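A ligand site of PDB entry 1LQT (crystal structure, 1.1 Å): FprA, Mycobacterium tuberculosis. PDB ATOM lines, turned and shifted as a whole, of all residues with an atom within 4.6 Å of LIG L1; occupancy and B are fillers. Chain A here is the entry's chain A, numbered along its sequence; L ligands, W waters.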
ATOM      1  N   HIS A  57      13.603 -24.817  -0.658  1.00  0.00           N
ATOM      2  CA  HIS A  57      14.073 -26.039   0.023  1.00  0.00           C
ATOM      3  C   HIS A  57      13.405 -26.123   1.421  1.00  0.00           C
ATOM      4  O   HIS A  57      14.076 -26.268   2.455  1.00  0.00           O
ATOM      5  CB  HIS A  57      15.614 -26.046   0.185  1.00  0.00           C
ATOM      6  CG  HIS A  57      16.367 -26.412  -1.062  1.00  0.00           C
ATOM      7  ND1 HIS A  57      17.670 -26.055  -1.262  1.00  0.00           N
ATOM      8  CD2 HIS A  57      16.051 -27.250  -2.081  1.00  0.00           C
ATOM      9  CE1 HIS A  57      18.083 -26.536  -2.427  1.00  0.00           C
ATOM     10  NE2 HIS A  57      17.115 -27.246  -2.955  1.00  0.00           N
ATOM     11  N   ARG A 110      33.925 -15.036   1.256  1.00  0.00           N
ATOM     12  CA  ARG A 110      35.216 -15.058   0.574  1.00  0.00           C
ATOM     13  C   ARG A 110      35.122 -14.193  -0.683  1.00  0.00           C
ATOM     14  O   ARG A 110      34.145 -14.213  -1.441  1.00  0.00           O
ATOM     15  CB  ARG A 110      35.605 -16.464   0.195  1.00  0.00           C
ATOM     16  CG  ARG A 110      35.906 -17.352   1.376  1.00  0.00           C
ATOM     17  CD  ARG A 110      36.523 -18.675   1.005  1.00  0.00           C
ATOM     18  NE  ARG A 110      37.877 -18.513   0.491  1.00  0.00           N
ATOM     19  CZ  ARG A 110      38.249 -18.595  -0.780  1.00  0.00           C
ATOM     20  NH1 ARG A 110      37.389 -18.754  -1.760  1.00  0.00           N
ATOM     21  NH2 ARG A 110      39.533 -18.443  -1.085  1.00  0.00           N
ATOM     22  N   LEU A 112      36.918 -12.773  -4.399  1.00  0.00           N
ATOM     23  CA  LEU A 112      37.703 -13.193  -5.544  1.00  0.00           C
ATOM     24  C   LEU A 112      39.056 -12.499  -5.624  1.00  0.00           C
ATOM     25  O   LEU A 112      39.989 -13.026  -6.223  1.00  0.00           O
ATOM     26  CB  LEU A 112      36.930 -12.852  -6.828  1.00  0.00           C
ATOM     27  CG  LEU A 112      35.591 -13.539  -6.990  1.00  0.00           C
ATOM     28  CD1 LEU A 112      34.828 -12.910  -8.135  1.00  0.00           C
ATOM     29  CD2 LEU A 112      35.739 -15.003  -7.193  1.00  0.00           C
ATOM     30  N   ILE A 153      29.842 -17.199  -9.815  1.00  0.00           N
ATOM     31  CA  ILE A 153      31.159 -17.833  -9.709  1.00  0.00           C
ATOM     32  C   ILE A 153      31.112 -18.888  -8.621  1.00  0.00           C
ATOM     33  O   ILE A 153      30.687 -18.593  -7.514  1.00  0.00           O
ATOM     34  CB  ILE A 153      32.255 -16.814  -9.382  1.00  0.00           C
ATOM     35  CG1 ILE A 153      32.216 -15.598 -10.308  1.00  0.00           C
ATOM     36  CG2 ILE A 153      33.607 -17.498  -9.375  1.00  0.00           C
ATOM     37  CD1 ILE A 153      32.365 -15.886 -11.777  1.00  0.00           C
ATOM     38  N   GLY A 154      31.545 -20.106  -8.938  1.00  0.00           N
ATOM     39  CA  GLY A 154      31.677 -21.173  -7.976  1.00  0.00           C
ATOM     40  C   GLY A 154      30.902 -22.412  -8.365  1.00  0.00           C
ATOM     41  O   GLY A 154      29.970 -22.350  -9.165  1.00  0.00           O
ATOM     42  N   ASN A 155      31.308 -23.528  -7.786  1.00  0.00           N
ATOM     43  CA  ASN A 155      30.731 -24.836  -8.071  1.00  0.00           C
ATOM     44  C   ASN A 155      30.332 -25.586  -6.809  1.00  0.00           C
ATOM     45  O   ASN A 155      30.461 -26.803  -6.753  1.00  0.00           O
ATOM     46  CB  ASN A 155      31.693 -25.691  -8.928  1.00  0.00           C
ATOM     47  CG  ASN A 155      31.621 -25.461 -10.446  1.00  0.00           C
ATOM     48  OD1 ASN A 155      32.369 -26.152 -11.133  1.00  0.00           O
ATOM     49  ND2 ASN A 155      30.810 -24.543 -10.947  1.00  0.00           N
ATOM     50  N   GLY A 156      29.803 -24.862  -5.822  1.00  0.00           N
ATOM     51  CA  GLY A 156      29.156 -25.479  -4.693  1.00  0.00           C
ATOM     52  C   GLY A 156      27.652 -25.355  -4.769  1.00  0.00           C
ATOM     53  O   GLY A 156      27.094 -24.694  -5.658  1.00  0.00           O
ATOM     54  N   ASN A 157      26.976 -25.993  -3.838  1.00  0.00           N
ATOM     55  CA  ASN A 157      25.530 -25.963  -3.867  1.00  0.00           C
ATOM     56  C   ASN A 157      24.953 -24.570  -3.676  1.00  0.00           C
ATOM     57  O   ASN A 157      23.849 -24.316  -4.128  1.00  0.00           O
ATOM     58  CB  ASN A 157      24.956 -26.934  -2.831  1.00  0.00           C
ATOM     59  CG  ASN A 157      25.111 -28.382  -3.217  1.00  0.00           C
ATOM     60  OD1 ASN A 157      25.086 -28.748  -4.380  1.00  0.00           O
ATOM     61  ND2 ASN A 157      25.232 -29.236  -2.209  1.00  0.00           N
ATOM     62  N   VAL A 158      25.662 -23.673  -3.008  1.00  0.00           N
ATOM     63  CA  VAL A 158      25.098 -22.329  -2.873  1.00  0.00           C
ATOM     64  C   VAL A 158      25.002 -21.656  -4.260  1.00  0.00           C
ATOM     65  O   VAL A 158      24.108 -20.886  -4.531  1.00  0.00           O
ATOM     66  CB  VAL A 158      25.872 -21.483  -1.857  1.00  0.00           C
ATOM     67  CG1 VAL A 158      25.354 -20.053  -1.828  1.00  0.00           C
ATOM     68  CG2 VAL A 158      25.780 -22.115  -0.484  1.00  0.00           C
ATOM     69  N   ALA A 159      25.955 -21.951  -5.152  1.00  0.00           N
ATOM     70  CA  ALA A 159      25.875 -21.422  -6.510  1.00  0.00           C
ATOM     71  C   ALA A 159      24.590 -21.878  -7.206  1.00  0.00           C
ATOM     72  O   ALA A 159      23.963 -21.120  -7.920  1.00  0.00           O
ATOM     73  CB  ALA A 159      27.073 -21.830  -7.330  1.00  0.00           C
ATOM     74  N   ASP A 161      21.779 -22.684  -5.600  1.00  0.00           N
ATOM     75  CA  ASP A 161      20.680 -21.956  -4.967  1.00  0.00           C
ATOM     76  C   ASP A 161      20.522 -20.579  -5.625  1.00  0.00           C
ATOM     77  O   ASP A 161      19.422 -20.155  -5.956  1.00  0.00           O
ATOM     78  CB  ASP A 161      20.916 -21.759  -3.479  1.00  0.00           C
ATOM     79  CG  ASP A 161      20.686 -22.972  -2.607  1.00  0.00           C
ATOM     80  OD1 ASP A 161      20.262 -24.016  -3.107  1.00  0.00           O
ATOM     81  OD2 ASP A 161      20.894 -22.871  -1.379  1.00  0.00           O
ATOM     82  N   ARG A 199      36.031 -22.905 -11.642  1.00  0.00           N
ATOM     83  CA  ARG A 199      37.443 -22.785 -11.972  1.00  0.00           C
ATOM     84  C   ARG A 199      38.105 -24.103 -12.296  1.00  0.00           C
ATOM     85  O   ARG A 199      38.999 -24.146 -13.167  1.00  0.00           O
ATOM     86  CB  ARG A 199      38.209 -22.009 -10.895  1.00  0.00           C
ATOM     87  CG  ARG A 199      38.292 -22.689  -9.525  1.00  0.00           C
ATOM     88  CD  ARG A 199      39.208 -21.943  -8.615  1.00  0.00           C
ATOM     89  NE  ARG A 199      39.164 -22.512  -7.272  1.00  0.00           N
ATOM     90  CZ  ARG A 199      39.790 -21.971  -6.249  1.00  0.00           C
ATOM     91  NH1 ARG A 199      40.509 -20.876  -6.424  1.00  0.00           N
ATOM     92  NH2 ARG A 199      39.709 -22.527  -5.064  1.00  0.00           N
ATOM     93  N   ARG A 200      37.711 -25.164 -11.591  1.00  0.00           N
ATOM     94  CA  ARG A 200      38.179 -26.507 -11.897  1.00  0.00           C
ATOM     95  C   ARG A 200      37.143 -27.202 -12.771  1.00  0.00           C
ATOM     96  O   ARG A 200      36.343 -26.551 -13.406  1.00  0.00           O
ATOM     97  CB  ARG A 200      38.593 -27.250 -10.622  1.00  0.00           C
ATOM     98  CG  ARG A 200      39.783 -26.578  -9.920  1.00  0.00           C
ATOM     99  CD  ARG A 200      40.403 -27.402  -8.829  1.00  0.00           C
ATOM    100  NE  ARG A 200      39.485 -27.573  -7.713  1.00  0.00           N
ATOM    101  CZ  ARG A 200      39.589 -28.525  -6.807  1.00  0.00           C
ATOM    102  NH1 ARG A 200      40.543 -29.442  -6.884  1.00  0.00           N
ATOM    103  NH2 ARG A 200      38.694 -28.614  -5.849  1.00  0.00           N
ATOM    104  N   GLN A 204      35.795 -32.002  -9.951  1.00  0.00           N
ATOM    105  CA  GLN A 204      36.157 -31.261  -8.757  1.00  0.00           C
ATOM    106  C   GLN A 204      34.977 -30.467  -8.183  1.00  0.00           C
ATOM    107  O   GLN A 204      35.121 -29.786  -7.186  1.00  0.00           O
ATOM    108  CB  GLN A 204      37.317 -30.330  -9.064  1.00  0.00           C
ATOM    109  CG  GLN A 204      38.602 -31.048  -9.360  1.00  0.00           C
ATOM    110  CD  GLN A 204      38.688 -31.592 -10.766  1.00  0.00           C
ATOM    111  OE1 GLN A 204      38.219 -30.954 -11.724  1.00  0.00           O
ATOM    112  NE2 GLN A 204      39.287 -32.773 -10.894  1.00  0.00           N
ATOM    113  N   ALA A 206      31.823 -29.200  -6.172  1.00  0.00           N
ATOM    114  CA  ALA A 206      31.367 -29.428  -4.797  1.00  0.00           C
ATOM    115  C   ALA A 206      29.847 -29.657  -4.735  1.00  0.00           C
ATOM    116  O   ALA A 206      29.293 -29.890  -3.661  1.00  0.00           O
ATOM    117  CB  ALA A 206      31.801 -28.303  -3.875  1.00  0.00           C
ATOM    118  N   THR A 208      26.227 -31.460  -4.968  1.00  0.00           N
ATOM    119  CA  THR A 208      25.742 -32.803  -4.679  1.00  0.00           C
ATOM    120  C   THR A 208      24.582 -33.141  -5.621  1.00  0.00           C
ATOM    121  O   THR A 208      24.041 -32.306  -6.310  1.00  0.00           O
ATOM    122  CB  THR A 208      25.452 -33.020  -3.183  1.00  0.00           C
ATOM    123  OG1 THR A 208      24.611 -31.977  -2.691  1.00  0.00           O
ATOM    124  CG2 THR A 208      26.755 -32.967  -2.397  1.00  0.00           C
ATOM    125  N   GLU A 211      20.646 -31.934  -5.730  1.00  0.00           N
ATOM    126  CA  GLU A 211      20.591 -30.540  -6.070  1.00  0.00           C
ATOM    127  C   GLU A 211      20.815 -30.326  -7.570  1.00  0.00           C
ATOM    128  O   GLU A 211      20.192 -29.479  -8.184  1.00  0.00           O
ATOM    129  CB  GLU A 211      21.586 -29.787  -5.211  1.00  0.00           C
ATOM    130  CG  GLU A 211      21.158 -29.813  -3.731  1.00  0.00           C
ATOM    131  CD  GLU A 211      21.245 -31.177  -2.990  1.00  0.00           C
ATOM    132  OE1 GLU A 211      22.088 -32.079  -3.367  1.00  0.00           O
ATOM    133  OE2 GLU A 211      20.456 -31.380  -1.985  1.00  0.00           O
ATOM    134  N   SER A 321      29.962 -16.986  -5.449  1.00  0.00           N
ATOM    135  CA  SER A 321      29.599 -18.049  -4.505  1.00  0.00           C
ATOM    136  C   SER A 321      30.825 -18.906  -4.290  1.00  0.00           C
ATOM    137  O   SER A 321      30.865 -20.081  -4.642  1.00  0.00           O
ATOM    138  CB  SER A 321      28.377 -18.824  -4.996  1.00  0.00           C
ATOM    139  OG  SER A 321      27.918 -19.671  -3.961  1.00  0.00           O
ATOM    140  N   VAL A 322      31.839 -18.295  -3.710  1.00  0.00           N
ATOM    141  CA  VAL A 322      33.127 -18.921  -3.540  1.00  0.00           C
ATOM    142  C   VAL A 322      33.417 -19.227  -2.090  1.00  0.00           C
ATOM    143  O   VAL A 322      34.568 -19.391  -1.686  1.00  0.00           O
ATOM    144  CB  VAL A 322      34.264 -18.210  -4.284  1.00  0.00           C
ATOM    145  CG1 VAL A 322      33.955 -18.164  -5.754  1.00  0.00           C
ATOM    146  CG2 VAL A 322      34.517 -16.792  -3.753  1.00  0.00           C
ATOM    147  N   GLY A 323      32.360 -19.319  -1.308  1.00  0.00           N
ATOM    148  CA  GLY A 323      32.424 -19.702   0.092  1.00  0.00           C
ATOM    149  C   GLY A 323      32.038 -18.600   1.026  1.00  0.00           C
ATOM    150  O   GLY A 323      32.273 -17.418   0.774  1.00  0.00           O
ATOM    151  N   TYR A 324      31.430 -19.018   2.125  1.00  0.00           N
ATOM    152  CA  TYR A 324      31.214 -18.158   3.283  1.00  0.00           C
ATOM    153  C   TYR A 324      32.578 -18.036   4.019  1.00  0.00           C
ATOM    154  O   TYR A 324      33.511 -18.745   3.700  1.00  0.00           O
ATOM    155  CB  TYR A 324      30.125 -18.725   4.190  1.00  0.00           C
ATOM    156  CG  TYR A 324      28.711 -18.436   3.686  1.00  0.00           C
ATOM    157  CD1 TYR A 324      28.281 -18.736   2.391  1.00  0.00           C
ATOM    158  CD2 TYR A 324      27.788 -17.884   4.548  1.00  0.00           C
ATOM    159  CE1 TYR A 324      26.994 -18.429   1.978  1.00  0.00           C
ATOM    160  CE2 TYR A 324      26.478 -17.577   4.141  1.00  0.00           C
ATOM    161  CZ  TYR A 324      26.097 -17.837   2.855  1.00  0.00           C
ATOM    162  OH  TYR A 324      24.844 -17.552   2.398  1.00  0.00           O
ATOM    163  N   TRP A 359      30.603 -24.287  11.800  1.00  0.00           N
ATOM    164  CA  TRP A 359      31.442 -23.673  10.769  1.00  0.00           C
ATOM    165  C   TRP A 359      32.544 -22.770  11.293  1.00  0.00           C
ATOM    166  O   TRP A 359      33.558 -22.648  10.613  1.00  0.00           O
ATOM    167  CB  TRP A 359      30.531 -22.955   9.764  1.00  0.00           C
ATOM    168  CG  TRP A 359      29.821 -23.908   8.851  1.00  0.00           C
ATOM    169  CD1 TRP A 359      29.757 -25.254   8.946  1.00  0.00           C
ATOM    170  CD2 TRP A 359      29.141 -23.551   7.655  1.00  0.00           C
ATOM    171  NE1 TRP A 359      29.076 -25.769   7.858  1.00  0.00           N
ATOM    172  CE2 TRP A 359      28.714 -24.736   7.040  1.00  0.00           C
ATOM    173  CE3 TRP A 359      28.894 -22.338   6.994  1.00  0.00           C
ATOM    174  CZ2 TRP A 359      28.074 -24.756   5.824  1.00  0.00           C
ATOM    175  CZ3 TRP A 359      28.251 -22.366   5.748  1.00  0.00           C
ATOM    176  CH2 TRP A 359      27.859 -23.570   5.198  1.00  0.00           C
ATOM    177  N   PRO A 364      33.499 -23.527   6.535  1.00  0.00           N
ATOM    178  CA  PRO A 364      32.125 -23.431   6.062  1.00  0.00           C
ATOM    179  C   PRO A 364      31.728 -24.492   5.089  1.00  0.00           C
ATOM    180  O   PRO A 364      31.330 -24.159   3.944  1.00  0.00           O
ATOM    181  CB  PRO A 364      32.111 -22.073   5.404  1.00  0.00           C
ATOM    182  CG  PRO A 364      33.476 -21.936   4.830  1.00  0.00           C
ATOM    183  CD  PRO A 364      34.386 -22.553   5.879  1.00  0.00           C
ATOM    184  N   THR A 365      31.780 -25.734   5.538  1.00  0.00           N
ATOM    185  CA  THR A 365      31.321 -26.815   4.679  1.00  0.00           C
ATOM    186  C   THR A 365      30.564 -27.864   5.497  1.00  0.00           C
ATOM    187  O   THR A 365      30.761 -28.057   6.700  1.00  0.00           O
ATOM    188  CB  THR A 365      32.410 -27.437   3.832  1.00  0.00           C
ATOM    189  OG1 THR A 365      33.359 -27.988   4.729  1.00  0.00           O
ATOM    190  CG2 THR A 365      33.151 -26.455   2.952  1.00  0.00           C
ATOM    191  N   GLY A 366      29.627 -28.474   4.822  1.00  0.00           N
ATOM    192  CA  GLY A 366      28.837 -29.555   5.339  1.00  0.00           C
ATOM    193  C   GLY A 366      27.368 -29.209   5.450  1.00  0.00           C
ATOM    194  O   GLY A 366      26.988 -28.075   5.773  1.00  0.00           O
ATOM    195  N   VAL A 367      26.554 -30.226   5.244  1.00  0.00           N
ATOM    196  CA  VAL A 367      25.130 -30.140   5.454  1.00  0.00           C
ATOM    197  C   VAL A 367      24.833 -29.977   6.958  1.00  0.00           C
ATOM    198  O   VAL A 367      25.699 -30.148   7.823  1.00  0.00           O
ATOM    199  CB  VAL A 367      24.403 -31.369   4.898  1.00  0.00           C
ATOM    200  CG1 VAL A 367      24.522 -31.412   3.387  1.00  0.00           C
ATOM    201  CG2 VAL A 367      24.874 -32.669   5.496  1.00  0.00           C
HETATM  202  O1  LIG L   1      38.122 -25.216  -6.931  1.00  0.00           O
HETATM  203  P1  LIG L   1      37.306 -25.269  -5.675  1.00  0.00           P
HETATM  204  O2  LIG L   1      36.767 -26.636  -5.343  1.00  0.00           O
HETATM  205  O3  LIG L   1      38.015 -24.630  -4.481  1.00  0.00           O
HETATM  206  O4  LIG L   1      36.038 -24.330  -6.032  1.00  0.00           O
HETATM  207  C1  LIG L   1      35.195 -23.765  -5.040  1.00  0.00           C
HETATM  208  C2  LIG L   1      33.838 -24.414  -4.904  1.00  0.00           C
HETATM  209  O5  LIG L   1      33.334 -24.764  -6.183  1.00  0.00           O
HETATM  210  C3  LIG L   1      34.833 -22.382  -5.438  1.00  0.00           C
HETATM  211  N1  LIG L   1      35.858 -21.380  -5.328  1.00  0.00           N
HETATM  212  C4  LIG L   1      36.563 -20.989  -4.215  1.00  0.00           C
HETATM  213  N2  LIG L   1      37.386 -19.984  -4.469  1.00  0.00           N
HETATM  214  C5  LIG L   1      37.211 -19.685  -5.797  1.00  0.00           C
HETATM  215  C6  LIG L   1      36.264 -20.556  -6.334  1.00  0.00           C
HETATM  216  N3  LIG L   1      35.819 -20.550  -7.618  1.00  0.00           N
HETATM  217  C7  LIG L   1      36.404 -19.602  -8.385  1.00  0.00           C
HETATM  218  N4  LIG L   1      37.321 -18.701  -7.946  1.00  0.00           N
HETATM  219  C8  LIG L   1      37.735 -18.730  -6.639  1.00  0.00           C
HETATM  220  N5  LIG L   1      38.597 -17.781  -6.253  1.00  0.00           N
HETATM  221  O6  LIG L   1      33.770 -22.064  -4.558  1.00  0.00           O
HETATM  222  C9  LIG L   1      33.000 -23.259  -4.351  1.00  0.00           C
HETATM  223  C10 LIG L   1      32.697 -23.404  -2.888  1.00  0.00           C
HETATM  224  O7  LIG L   1      31.801 -24.483  -2.737  1.00  0.00           O
HETATM  225  P2  LIG L   1      31.483 -25.032  -1.273  1.00  0.00           P
HETATM  226  O8  LIG L   1      30.618 -26.200  -1.427  1.00  0.00           O
HETATM  227  O9  LIG L   1      32.723 -25.187  -0.481  1.00  0.00           O
HETATM  228  O10 LIG L   1      30.718 -23.805  -0.604  1.00  0.00           O
HETATM  229  P3  LIG L   1      29.189 -23.264  -0.703  1.00  0.00           P
HETATM  230  O11 LIG L   1      28.650 -23.437  -2.065  1.00  0.00           O
HETATM  231  O12 LIG L   1      29.261 -21.919  -0.087  1.00  0.00           O
HETATM  232  O13 LIG L   1      28.398 -24.266   0.228  1.00  0.00           O
HETATM  233  C11 LIG L   1      28.716 -24.291   1.644  1.00  0.00           C
HETATM  234  C12 LIG L   1      28.213 -25.593   2.218  1.00  0.00           C
HETATM  235  O14 LIG L   1      26.799 -25.615   2.362  1.00  0.00           O
HETATM  236  C13 LIG L   1      26.266 -26.767   1.717  1.00  0.00           C
HETATM  237  C14 LIG L   1      27.294 -27.144   0.724  1.00  0.00           C
HETATM  238  O15 LIG L   1      27.134 -28.389   0.140  1.00  0.00           O
HETATM  239  C15 LIG L   1      28.589 -26.798   1.368  1.00  0.00           C
HETATM  240  O16 LIG L   1      28.994 -27.886   2.173  1.00  0.00           O
HETATM  241  N6  LIG L   1      24.917 -26.585   1.316  1.00  0.00           N
HETATM  242  C16 LIG L   1      24.138 -27.753   1.139  1.00  0.00           C
HETATM  243  C17 LIG L   1      23.003 -27.657   0.395  1.00  0.00           C
HETATM  244  C18 LIG L   1      22.263 -28.993   0.245  1.00  0.00           C
HETATM  245  N7  LIG L   1      21.171 -28.951  -0.476  1.00  0.00           N
HETATM  246  O17 LIG L   1      22.754 -30.007   0.795  1.00  0.00           O
HETATM  247  C19 LIG L   1      22.578 -26.485  -0.241  1.00  0.00           C
HETATM  248  O18 LIG L   1      21.550 -26.418  -0.982  1.00  0.00           O
HETATM  249  C20 LIG L   1      23.426 -25.306  -0.065  1.00  0.00           C
HETATM  250  C21 LIG L   1      24.600 -25.384   0.706  1.00  0.00           C
HETATM  251  P1  LG2 L   2      24.921 -20.960  11.406  1.00  0.00           P
HETATM  252  O1  LG2 L   2      25.439 -19.914  10.506  1.00  0.00           O
HETATM  253  O2  LG2 L   2      23.760 -21.797  10.989  1.00  0.00           O
HETATM  254  O3  LG2 L   2      24.509 -20.288  12.802  1.00  0.00           O
HETATM  255  C1  LG2 L   2      25.350 -19.280  13.374  1.00  0.00           C
HETATM  256  C2  LG2 L   2      24.463 -18.453  14.303  1.00  0.00           C
HETATM  257  O4  LG2 L   2      25.327 -17.651  15.103  1.00  0.00           O
HETATM  258  C3  LG2 L   2      23.513 -17.507  13.575  1.00  0.00           C
HETATM  259  O5  LG2 L   2      22.194 -17.584  14.061  1.00  0.00           O
HETATM  260  C4  LG2 L   2      24.148 -16.164  13.798  1.00  0.00           C
HETATM  261  O6  LG2 L   2      23.274 -15.051  13.725  1.00  0.00           O
HETATM  262  C5  LG2 L   2      24.778 -16.351  15.189  1.00  0.00           C
HETATM  263  N1  LG2 L   2      25.849 -15.418  15.493  1.00  0.00           N
HETATM  264  C6  LG2 L   2      26.915 -15.118  14.694  1.00  0.00           C
HETATM  265  N2  LG2 L   2      27.744 -14.245  15.273  1.00  0.00           N
HETATM  266  C7  LG2 L   2      27.155 -13.956  16.490  1.00  0.00           C
HETATM  267  C8  LG2 L   2      27.542 -13.102  17.517  1.00  0.00           C
HETATM  268  N3  LG2 L   2      28.662 -12.397  17.516  1.00  0.00           N
HETATM  269  N4  LG2 L   2      26.730 -13.041  18.611  1.00  0.00           N
HETATM  270  C9  LG2 L   2      25.607 -13.806  18.653  1.00  0.00           C
HETATM  271  N5  LG2 L   2      25.180 -14.651  17.703  1.00  0.00           N
HETATM  272  C10 LG2 L   2      25.991 -14.687  16.642  1.00  0.00           C
HETATM  273  N6  LG2 L   2      22.575 -27.677   4.752  1.00  0.00           N
HETATM  274  C11 LG2 L   2      21.666 -28.662   4.501  1.00  0.00           C
HETATM  275  O7  LG2 L   2      21.678 -29.708   5.114  1.00  0.00           O
HETATM  276  N7  LG2 L   2      20.717 -28.456   3.500  1.00  0.00           N
HETATM  277  C12 LG2 L   2      20.582 -27.289   2.804  1.00  0.00           C
HETATM  278  O8  LG2 L   2      19.687 -27.161   1.939  1.00  0.00           O
HETATM  279  C13 LG2 L   2      21.491 -26.276   3.110  1.00  0.00           C
HETATM  280  N8  LG2 L   2      21.410 -25.055   2.462  1.00  0.00           N
HETATM  281  C14 LG2 L   2      22.326 -24.078   2.741  1.00  0.00           C
HETATM  282  C15 LG2 L   2      22.271 -22.874   2.085  1.00  0.00           C
HETATM  283  C16 LG2 L   2      23.214 -21.884   2.274  1.00  0.00           C
HETATM  284  C17 LG2 L   2      23.105 -20.574   1.538  1.00  0.00           C
HETATM  285  C18 LG2 L   2      24.246 -22.124   3.189  1.00  0.00           C
HETATM  286  C19 LG2 L   2      25.318 -21.085   3.424  1.00  0.00           C
HETATM  287  C20 LG2 L   2      24.305 -23.321   3.890  1.00  0.00           C
HETATM  288  C21 LG2 L   2      23.357 -24.320   3.670  1.00  0.00           C
HETATM  289  N9  LG2 L   2      23.416 -25.543   4.338  1.00  0.00           N
HETATM  290  C22 LG2 L   2      22.473 -26.505   4.081  1.00  0.00           C
HETATM  291  C23 LG2 L   2      24.450 -25.830   5.382  1.00  0.00           C
HETATM  292  C24 LG2 L   2      23.979 -25.381   6.768  1.00  0.00           C
HETATM  293  O9  LG2 L   2      23.436 -24.092   6.651  1.00  0.00           O
HETATM  294  C25 LG2 L   2      25.174 -25.380   7.739  1.00  0.00           C
HETATM  295  O10 LG2 L   2      25.719 -26.689   7.881  1.00  0.00           O
HETATM  296  C26 LG2 L   2      24.849 -24.968   9.172  1.00  0.00           C
HETATM  297  O11 LG2 L   2      23.831 -23.971   9.214  1.00  0.00           O
HETATM  298  C27 LG2 L   2      26.110 -24.465   9.881  1.00  0.00           C
HETATM  299  O12 LG2 L   2      25.733 -24.315  11.256  1.00  0.00           O
HETATM  300  P2  LG2 L   2      26.447 -23.348  12.294  1.00  0.00           P
HETATM  301  O13 LG2 L   2      25.712 -23.574  13.557  1.00  0.00           O
HETATM  302  O14 LG2 L   2      27.937 -23.510  12.313  1.00  0.00           O
HETATM  303  O15 LG2 L   2      26.210 -21.874  11.753  1.00  0.00           O
HETATM  304  O   HOH W   1      39.898 -26.060  -3.104  1.00  0.00           O
HETATM  305  O   HOH W   2      39.146 -18.224 -10.007  1.00  0.00           O
HETATM  306  O   HOH W   3      35.967 -27.803  -3.148  1.00  0.00           O
HETATM  307  O   HOH W   4      34.497 -27.079  -6.707  1.00  0.00           O
HETATM  308  O   HOH W   5      37.101 -24.035  -1.933  1.00  0.00           O
HETATM  309  O   HOH W   6      30.962 -21.775   2.152  1.00  0.00           O
HETATM  310  O   HOH W   7      29.394 -19.439  -1.364  1.00  0.00           O
HETATM  311  O   HOH W   8      27.347 -31.296   1.030  1.00  0.00           O
HETATM  312  O   HOH W   9      21.577 -26.410  -3.876  1.00  0.00           O
HETATM  313  O   HOH W  10      24.749 -31.714   0.092  1.00  0.00           O
HETATM  314  O   HOH W  11      28.503 -27.708  -2.107  1.00  0.00           O
HETATM  315  O   HOH W  12      34.637 -22.770  -9.019  1.00  0.00           O
HETATM  316  O   HOH W  13      29.121 -22.231  -4.456  1.00  0.00           O
HETATM  317  O   HOH W  14      33.353 -23.204   1.247  1.00  0.00           O
HETATM  318  O   HOH W  15      39.836 -15.452  -7.564  1.00  0.00           O
HETATM  319  O   HOH W  16      35.182 -25.973  -1.203  1.00  0.00           O
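The side-chain carboxylate (OD1) of Asp 161 sits close to an oxygen (O18) of LIG L1, 3.5 Å away.
Residues that only touch LIG L1: Val 322, Gly 156, Ala 206, Val 367, Pro 364, Ser 321, Thr 365, Trp 359, Ile 153, His 57 and Gly 323.
Hydrophobic or aromatic side chains within 4 Å of LIG L1: His 57, Ile 153, Val 158, Ala 206, Val 322, Trp 359 and Val 367.
Of the 26 residues printed, 20 come within 4 Å of LIG L1.
O of Asn 155 lies within hydrogen-bond range of N of Ala 206 (2.8 Å).
The side-chain hydroxyl (OG1) of Thr 208 is in hydrogen-bond range of the side-chain carboxylate (OE1) of Glu 211.
NH1 of Arg 110 lies within hydrogen-bond range of O of Val 322.
O of Gly 323 is in hydrogen-bond range of N of Arg 110 (2.9 Å).
The side-chain hydroxyl (OG1) of Thr 208 lies within hydrogen-bond range of the side-chain amide nitrogen (ND2) of Asn 157, 2.9 Å away.
N of Ser 321 is in hydrogen-bond range of O of Ile 153 (2.7 Å).
The side-chain hydroxyl (OG) of Ser 321 is in hydrogen-bond range of the backbone NH (N) of Ala 159 (3.2 Å).
O of Thr 365 is in hydrogen-bond range of NE1 of Trp 359 (3.1 Å).
An oxygen (O3) of LIG L1 is in salt-bridge range of the guanidinium group (NH2) of Arg 199 (2.8 Å).
The backbone NH of Gly 366 lies within hydrogen-bond range of an oxygen (O16) of LIG L1 (2.8 Å).
The guanidinium group (NH2) of Arg 200 is in salt-bridge range of an oxygen (O2) of LIG L1 (2.8 Å).
N of Asn 155 is in hydrogen-bond range of O5 of LIG L1, at 2.9 Å.
A nitrogen (N7) of LIG L1 sits at hydrogen-bond distance from the side-chain carboxylate (OE2) of Glu 211 (2.9 Å).
A nitrogen (N2) of LIG L1 lies within hydrogen-bond range of the guanidinium group (NH1) of Arg 110.
The side-chain amide nitrogen (ND2) of Asn 157 is in hydrogen-bond range of an oxygen (O15) of LIG L1, at 3.1 Å.
The backbone NH of Val 158 is in hydrogen-bond range of an oxygen (O11) of LIG L1, 3.1 Å away.
O of Gly 366 is in hydrogen-bond range of O10 of LG2 L2 (2.8 Å).
O of Val 367 is in hydrogen-bond range of O10 of LG2 L2, 3.5 Å away.
N of Trp 359 lies within hydrogen-bond range of O14 of LG2 L2, 2.8 Å away.
An oxygen (O10) of LG2 L2 lies within hydrogen-bond range of the indole nitrogen (NE1) of Trp 359, at 3.5 Å.
N7 of LIG L1 lies within hydrogen-bond range of O8 of LG2 L2, at 3.4 Å.
Water W4 lies within hydrogen-bond range of an oxygen (O5) of LIG L1 (2.6 Å), the backbone carbonyl oxygen (O) of Gln 204 (2.8 Å) and the backbone NH (N) of Ala 206 (3.5 Å).
Water W11 lies within hydrogen-bond range of an oxygen (O8) of LIG L1 (2.7 Å), the backbone carbonyl oxygen of Ala 206 (2.8 Å) and the backbone NH of Asn 157 (2.9 Å).
Water W7 lies within hydrogen-bond range of O12 of LIG L1, N of Gly 323 and OG of Ser 321.
Water W6 lies within hydrogen-bond range of N of Tyr 324 (2.8 Å), O12 of LIG L1 (2.8 Å) and O of Pro 364 (3.0 Å).
Water W12 lies within hydrogen-bond range of a nitrogen (N3) of LIG L1 and the backbone NH (N) of Arg 199.
Water W15 bridges O of Leu 112 and N5 of LIG L1.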
